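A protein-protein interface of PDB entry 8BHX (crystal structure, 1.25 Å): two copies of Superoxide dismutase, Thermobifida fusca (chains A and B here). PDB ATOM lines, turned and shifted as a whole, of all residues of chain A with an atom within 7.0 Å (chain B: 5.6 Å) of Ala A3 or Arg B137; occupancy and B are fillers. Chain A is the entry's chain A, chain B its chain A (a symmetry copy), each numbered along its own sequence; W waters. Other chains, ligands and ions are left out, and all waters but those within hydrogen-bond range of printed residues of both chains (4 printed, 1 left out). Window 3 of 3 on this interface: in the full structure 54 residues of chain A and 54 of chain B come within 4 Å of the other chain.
NH1 of Arg B137 sits at hydrogen-bond distance from O of Ala A3 (3.3 Å). The side-chain hydroxyl (OH) of Tyr A5 lies within hydrogen-bond range of the side-chain carboxylate (OD2) of Asp B132 (2.6 Å).
Among the printed residues, pairs that only touch across the chains: Leu A45 with Arg B137, Ser A2 with Arg B137, Tyr A5 with Arg B137, Tyr A5 with Gly B135, Leu A71 with Ile B139 and Leu A71 with Asp B132.
Of chain B, only Arg B137 comes within 4 Å of Ala A3. Of the printed residues of chain B, Tyr A5 touches Asp B132, Gly B135 and Arg B137. Thr A6 touches none of the printed residues of chain B. Printed residues of chain B within 4 Å of Leu A45: Arg B137. Printed residues of chain B within 4 Å of Leu A71: Asp B132 (3.8 Å) and Ile B139 (3.8 Å). Of the printed residues of chain A, Asp B132 touches Tyr A5 (2.6 Å) and Leu A71 (3.8 Å). Of the printed residues of chain A, Gly B135 touches Tyr A5 (3.7 Å). Arg B137 touches just these residues of chain A: Ser A2 (3.5 Å), Ala A3 (3.3 Å), Tyr A5 (3.6 Å) and Leu A45 (3.5 Å). The nearest residue of chain B that does not touch Ala A3 is Gly B135 (5.2 Å).
Water W1 lies within hydrogen-bond range of the backbone carbonyl oxygen (O) of Gly B135 (2.6 Å) and the backbone carbonyl oxygen (O) of Ala A3 (3.2 Å). Water W4 lies within hydrogen-bond range of NH1 of Arg B137 (2.7 Å) and O of Ala A3 (2.7 Å). Water W2 lies within hydrogen-bond range of OD1 of Asn A42 (2.8 Å) and NH1 of Arg B137 (3.3 Å). Water W3 lies within hydrogen-bond range of the backbone carbonyl oxygen of Gln B136, the backbone carbonyl oxygen of Gly B135 and the side-chain hydroxyl of Ser A2.
N of Tyr A5 sits at hydrogen-bond distance from OD1 of Asn A42 (2.9 Å). O of Ile B139 is in hydrogen-bond range of N of Ala B130, 2.8 Å away. N of Gly B135 is in hydrogen-bond range of OD2 of Asp B132 (2.8 Å). O of Arg B137 lies within hydrogen-bond range of N of Asp B132 (2.8 Å).
No position is printed for both chains. Of the 8 pairs that touch across the chains among the printed residues, none has its exchanged pair printed and touching as well.
Hydrophobic or aromatic side chains of chain A that line the printed part of chain B: Tyr A5, Leu A45 and Leu A71. Of the 8 printed residues of chain B, 4 touch a printed residue of chain A. Hydrophobic or aromatic side chains of chain B within 4 Å of the printed part of chain A: Ile B139. Among the printed residues, 8 pairs touch across the chains.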
ATOM      1  N   SER A   2       7.571  -4.967   1.286  1.00  0.00           N
ATOM      2  CA  SER A   2       8.528  -3.925   0.933  1.00  0.00           C
ATOM      3  C   SER A   2       8.496  -2.798   1.961  1.00  0.00           C
ATOM      4  O   SER A   2       7.456  -2.518   2.561  1.00  0.00           O
ATOM      5  CB  SER A   2       8.221  -3.372  -0.462  1.00  0.00           C
ATOM      6  OG  SER A   2       8.394  -4.365  -1.456  1.00  0.00           O
ATOM      7  N   ALA A   3       9.638  -2.140   2.151  1.00  0.00           N
ATOM      8  CA  ALA A   3       9.721  -1.091   3.160  1.00  0.00           C
ATOM      9  C   ALA A   3       9.022   0.171   2.657  1.00  0.00           C
ATOM     10  O   ALA A   3       9.099   0.488   1.469  1.00  0.00           O
ATOM     11  CB  ALA A   3      11.179  -0.762   3.463  1.00  0.00           C
ATOM     12  N   PRO A   4       8.341   0.910   3.533  1.00  0.00           N
ATOM     13  CA  PRO A   4       7.713   2.161   3.089  1.00  0.00           C
ATOM     14  C   PRO A   4       8.741   3.164   2.595  1.00  0.00           C
ATOM     15  O   PRO A   4       9.906   3.157   3.003  1.00  0.00           O
ATOM     16  CB  PRO A   4       7.014   2.684   4.350  1.00  0.00           C
ATOM     17  CG  PRO A   4       6.872   1.495   5.244  1.00  0.00           C
ATOM     18  CD  PRO A   4       8.082   0.649   4.976  1.00  0.00           C
ATOM     19  N   TYR A   5       8.286   4.042   1.710  1.00  0.00           N
ATOM     20  CA  TYR A   5       9.102   5.169   1.291  1.00  0.00           C
ATOM     21  C   TYR A   5       9.401   6.053   2.496  1.00  0.00           C
ATOM     22  O   TYR A   5       8.591   6.168   3.417  1.00  0.00           O
ATOM     23  CB  TYR A   5       8.343   6.004   0.251  1.00  0.00           C
ATOM     24  CG  TYR A   5       8.038   5.259  -1.022  1.00  0.00           C
ATOM     25  CD1 TYR A   5       9.049   4.939  -1.914  1.00  0.00           C
ATOM     26  CD2 TYR A   5       6.737   4.879  -1.335  1.00  0.00           C
ATOM     27  CE1 TYR A   5       8.783   4.256  -3.084  1.00  0.00           C
ATOM     28  CE2 TYR A   5       6.465   4.200  -2.503  1.00  0.00           C
ATOM     29  CZ  TYR A   5       7.493   3.896  -3.378  1.00  0.00           C
ATOM     30  OH  TYR A   5       7.211   3.190  -4.543  1.00  0.00           O
ATOM     31  N   THR A   6      10.573   6.688   2.482  1.00  0.00           N
ATOM     32  CA  THR A   6      10.973   7.627   3.521  1.00  0.00           C
ATOM     33  C   THR A   6      11.546   8.897   2.899  1.00  0.00           C
ATOM     34  O   THR A   6      11.989   8.906   1.750  1.00  0.00           O
ATOM     35  CB  THR A   6      12.026   7.023   4.453  1.00  0.00           C
ATOM     36  OG1 THR A   6      13.172   6.667   3.681  1.00  0.00           O
ATOM     37  CG2 THR A   6      11.481   5.802   5.179  1.00  0.00           C
ATOM     38  N   ASN A  42       3.154   6.398   0.029  1.00  0.00           N
ATOM     39  CA  ASN A  42       2.807   5.300   0.921  1.00  0.00           C
ATOM     40  C   ASN A  42       1.300   5.151   1.035  1.00  0.00           C
ATOM     41  O   ASN A  42       0.769   4.030   0.985  1.00  0.00           O
ATOM     42  CB  ASN A  42       3.412   5.559   2.300  1.00  0.00           C
ATOM     43  CG  ASN A  42       4.899   5.334   2.325  1.00  0.00           C
ATOM     44  OD1 ASN A  42       5.404   4.421   1.682  1.00  0.00           O
ATOM     45  ND2 ASN A  42       5.612   6.139   3.110  1.00  0.00           N
ATOM     46  N   LEU A  45      -0.197   3.417  -2.082  1.00  0.00           N
ATOM     47  CA  LEU A  45       0.001   1.975  -2.091  1.00  0.00           C
ATOM     48  C   LEU A  45      -0.903   1.295  -1.072  1.00  0.00           C
ATOM     49  O   LEU A  45      -1.471   0.230  -1.357  1.00  0.00           O
ATOM     50  CB  LEU A  45       1.471   1.628  -1.849  1.00  0.00           C
ATOM     51  CG  LEU A  45       2.411   1.955  -3.013  1.00  0.00           C
ATOM     52  CD1 LEU A  45       3.842   1.734  -2.559  1.00  0.00           C
ATOM     53  CD2 LEU A  45       2.105   1.141  -4.265  1.00  0.00           C
ATOM     54  N   LEU A  71       4.577   9.335  -6.219  1.00  0.00           N
ATOM     55  CA  LEU A  71       5.834   8.620  -6.425  1.00  0.00           C
ATOM     56  C   LEU A  71       6.749   9.420  -7.341  1.00  0.00           C
ATOM     57  O   LEU A  71       7.947   9.532  -7.088  1.00  0.00           O
ATOM     58  CB  LEU A  71       5.592   7.211  -6.975  1.00  0.00           C
ATOM     59  CG  LEU A  71       6.868   6.422  -7.290  1.00  0.00           C
ATOM     60  CD1 LEU A  71       7.742   6.231  -6.063  1.00  0.00           C
ATOM     61  CD2 LEU A  71       6.528   5.062  -7.890  1.00  0.00           C
ATOM     62  N   ALA B 130       5.358  -2.424 -13.743  1.00  0.00           N
ATOM     63  CA  ALA B 130       6.674  -1.811 -13.796  1.00  0.00           C
ATOM     64  C   ALA B 130       7.400  -2.052 -12.483  1.00  0.00           C
ATOM     65  O   ALA B 130       6.798  -2.375 -11.454  1.00  0.00           O
ATOM     66  CB  ALA B 130       6.575  -0.299 -14.027  1.00  0.00           C
ATOM     67  N   TRP B 131       8.714  -1.884 -12.533  1.00  0.00           N
ATOM     68  CA  TRP B 131       9.549  -1.910 -11.340  1.00  0.00           C
ATOM     69  C   TRP B 131       9.898  -0.477 -10.969  1.00  0.00           C
ATOM     70  O   TRP B 131      10.478   0.251 -11.779  1.00  0.00           O
ATOM     71  CB  TRP B 131      10.823  -2.698 -11.619  1.00  0.00           C
ATOM     72  CG  TRP B 131      11.770  -2.902 -10.457  1.00  0.00           C
ATOM     73  CD1 TRP B 131      12.986  -2.318 -10.290  1.00  0.00           C
ATOM     74  CD2 TRP B 131      11.592  -3.788  -9.337  1.00  0.00           C
ATOM     75  NE1 TRP B 131      13.574  -2.788  -9.141  1.00  0.00           N
ATOM     76  CE2 TRP B 131      12.739  -3.685  -8.534  1.00  0.00           C
ATOM     77  CE3 TRP B 131      10.573  -4.657  -8.942  1.00  0.00           C
ATOM     78  CZ2 TRP B 131      12.897  -4.428  -7.354  1.00  0.00           C
ATOM     79  CZ3 TRP B 131      10.723  -5.376  -7.770  1.00  0.00           C
ATOM     80  CH2 TRP B 131      11.873  -5.260  -6.995  1.00  0.00           C
ATOM     81  N   ASP B 132       9.532  -0.069  -9.755  1.00  0.00           N
ATOM     82  CA  ASP B 132       9.942   1.232  -9.229  1.00  0.00           C
ATOM     83  C   ASP B 132      11.397   1.140  -8.801  1.00  0.00           C
ATOM     84  O   ASP B 132      11.722   0.393  -7.879  1.00  0.00           O
ATOM     85  CB  ASP B 132       9.064   1.602  -8.039  1.00  0.00           C
ATOM     86  CG  ASP B 132       9.614   2.771  -7.242  1.00  0.00           C
ATOM     87  OD1 ASP B 132      10.319   3.622  -7.832  1.00  0.00           O
ATOM     88  OD2 ASP B 132       9.333   2.808  -6.024  1.00  0.00           O
ATOM     89  N   GLY B 135      11.849   2.587  -4.806  1.00  0.00           N
ATOM     90  CA  GLY B 135      11.384   1.680  -3.771  1.00  0.00           C
ATOM     91  C   GLY B 135      11.737   0.223  -3.962  1.00  0.00           C
ATOM     92  O   GLY B 135      11.539  -0.565  -3.032  1.00  0.00           O
ATOM     93  N   GLN B 136      12.269  -0.151  -5.122  1.00  0.00           N
ATOM     94  CA  GLN B 136      12.639  -1.536  -5.409  1.00  0.00           C
ATOM     95  C   GLN B 136      11.441  -2.467  -5.214  1.00  0.00           C
ATOM     96  O   GLN B 136      11.461  -3.382  -4.388  1.00  0.00           O
ATOM     97  CB  GLN B 136      13.838  -1.955  -4.551  1.00  0.00           C
ATOM     98  CG  GLN B 136      15.113  -1.156  -4.830  1.00  0.00           C
ATOM     99  CD  GLN B 136      15.558  -1.308  -6.260  1.00  0.00           C
ATOM    100  OE1 GLN B 136      15.963  -0.336  -6.906  1.00  0.00           O
ATOM    101  NE2 GLN B 136      15.529  -2.524  -6.760  1.00  0.00           N
ATOM    102  N   ARG B 137      10.385  -2.205  -5.988  1.00  0.00           N
ATOM    103  CA  ARG B 137       9.125  -2.913  -5.811  1.00  0.00           C
ATOM    104  C   ARG B 137       8.300  -2.846  -7.082  1.00  0.00           C
ATOM    105  O   ARG B 137       8.445  -1.933  -7.898  1.00  0.00           O
ATOM    106  CB  ARG B 137       8.338  -2.343  -4.626  1.00  0.00           C
ATOM    107  CG  ARG B 137       7.876  -0.891  -4.811  1.00  0.00           C
ATOM    108  CD  ARG B 137       7.566  -0.273  -3.460  1.00  0.00           C
ATOM    109  NE  ARG B 137       6.439  -0.947  -2.832  1.00  0.00           N
ATOM    110  CZ  ARG B 137       6.069  -0.787  -1.569  1.00  0.00           C
ATOM    111  NH1 ARG B 137       6.733   0.047  -0.781  1.00  0.00           N
ATOM    112  NH2 ARG B 137       5.026  -1.463  -1.103  1.00  0.00           N
ATOM    113  N   LEU B 138       7.423  -3.835  -7.232  1.00  0.00           N
ATOM    114  CA  LEU B 138       6.496  -3.857  -8.356  1.00  0.00           C
ATOM    115  C   LEU B 138       5.349  -2.890  -8.132  1.00  0.00           C
ATOM    116  O   LEU B 138       4.799  -2.805  -7.029  1.00  0.00           O
ATOM    117  CB  LEU B 138       5.908  -5.252  -8.528  1.00  0.00           C
ATOM    118  CG  LEU B 138       6.864  -6.326  -9.012  1.00  0.00           C
ATOM    119  CD1 LEU B 138       6.152  -7.665  -8.954  1.00  0.00           C
ATOM    120  CD2 LEU B 138       7.320  -6.058 -10.429  1.00  0.00           C
ATOM    121  N   ILE B 139       4.969  -2.188  -9.199  1.00  0.00           N
ATOM    122  CA  ILE B 139       3.785  -1.334  -9.199  1.00  0.00           C
ATOM    123  C   ILE B 139       3.087  -1.490 -10.546  1.00  0.00           C
ATOM    124  O   ILE B 139       3.697  -1.875 -11.548  1.00  0.00           O
ATOM    125  CB  ILE B 139       4.109   0.160  -8.950  1.00  0.00           C
ATOM    126  CG1 ILE B 139       5.074   0.688 -10.019  1.00  0.00           C
ATOM    127  CG2 ILE B 139       4.700   0.376  -7.550  1.00  0.00           C
ATOM    128  CD1 ILE B 139       5.307   2.192  -9.979  1.00  0.00           C
HETATM  129  O   HOH W   1      11.262  -0.756  -0.476  1.00  0.00           O
HETATM  130  O   HOH W   2       4.711   1.697   1.316  1.00  0.00           O
HETATM  131  O   HOH W   3      11.641  -3.225  -1.348  1.00  0.00           O
HETATM  132  O   HOH W   4       8.907   1.554  -0.982  1.00  0.00           O
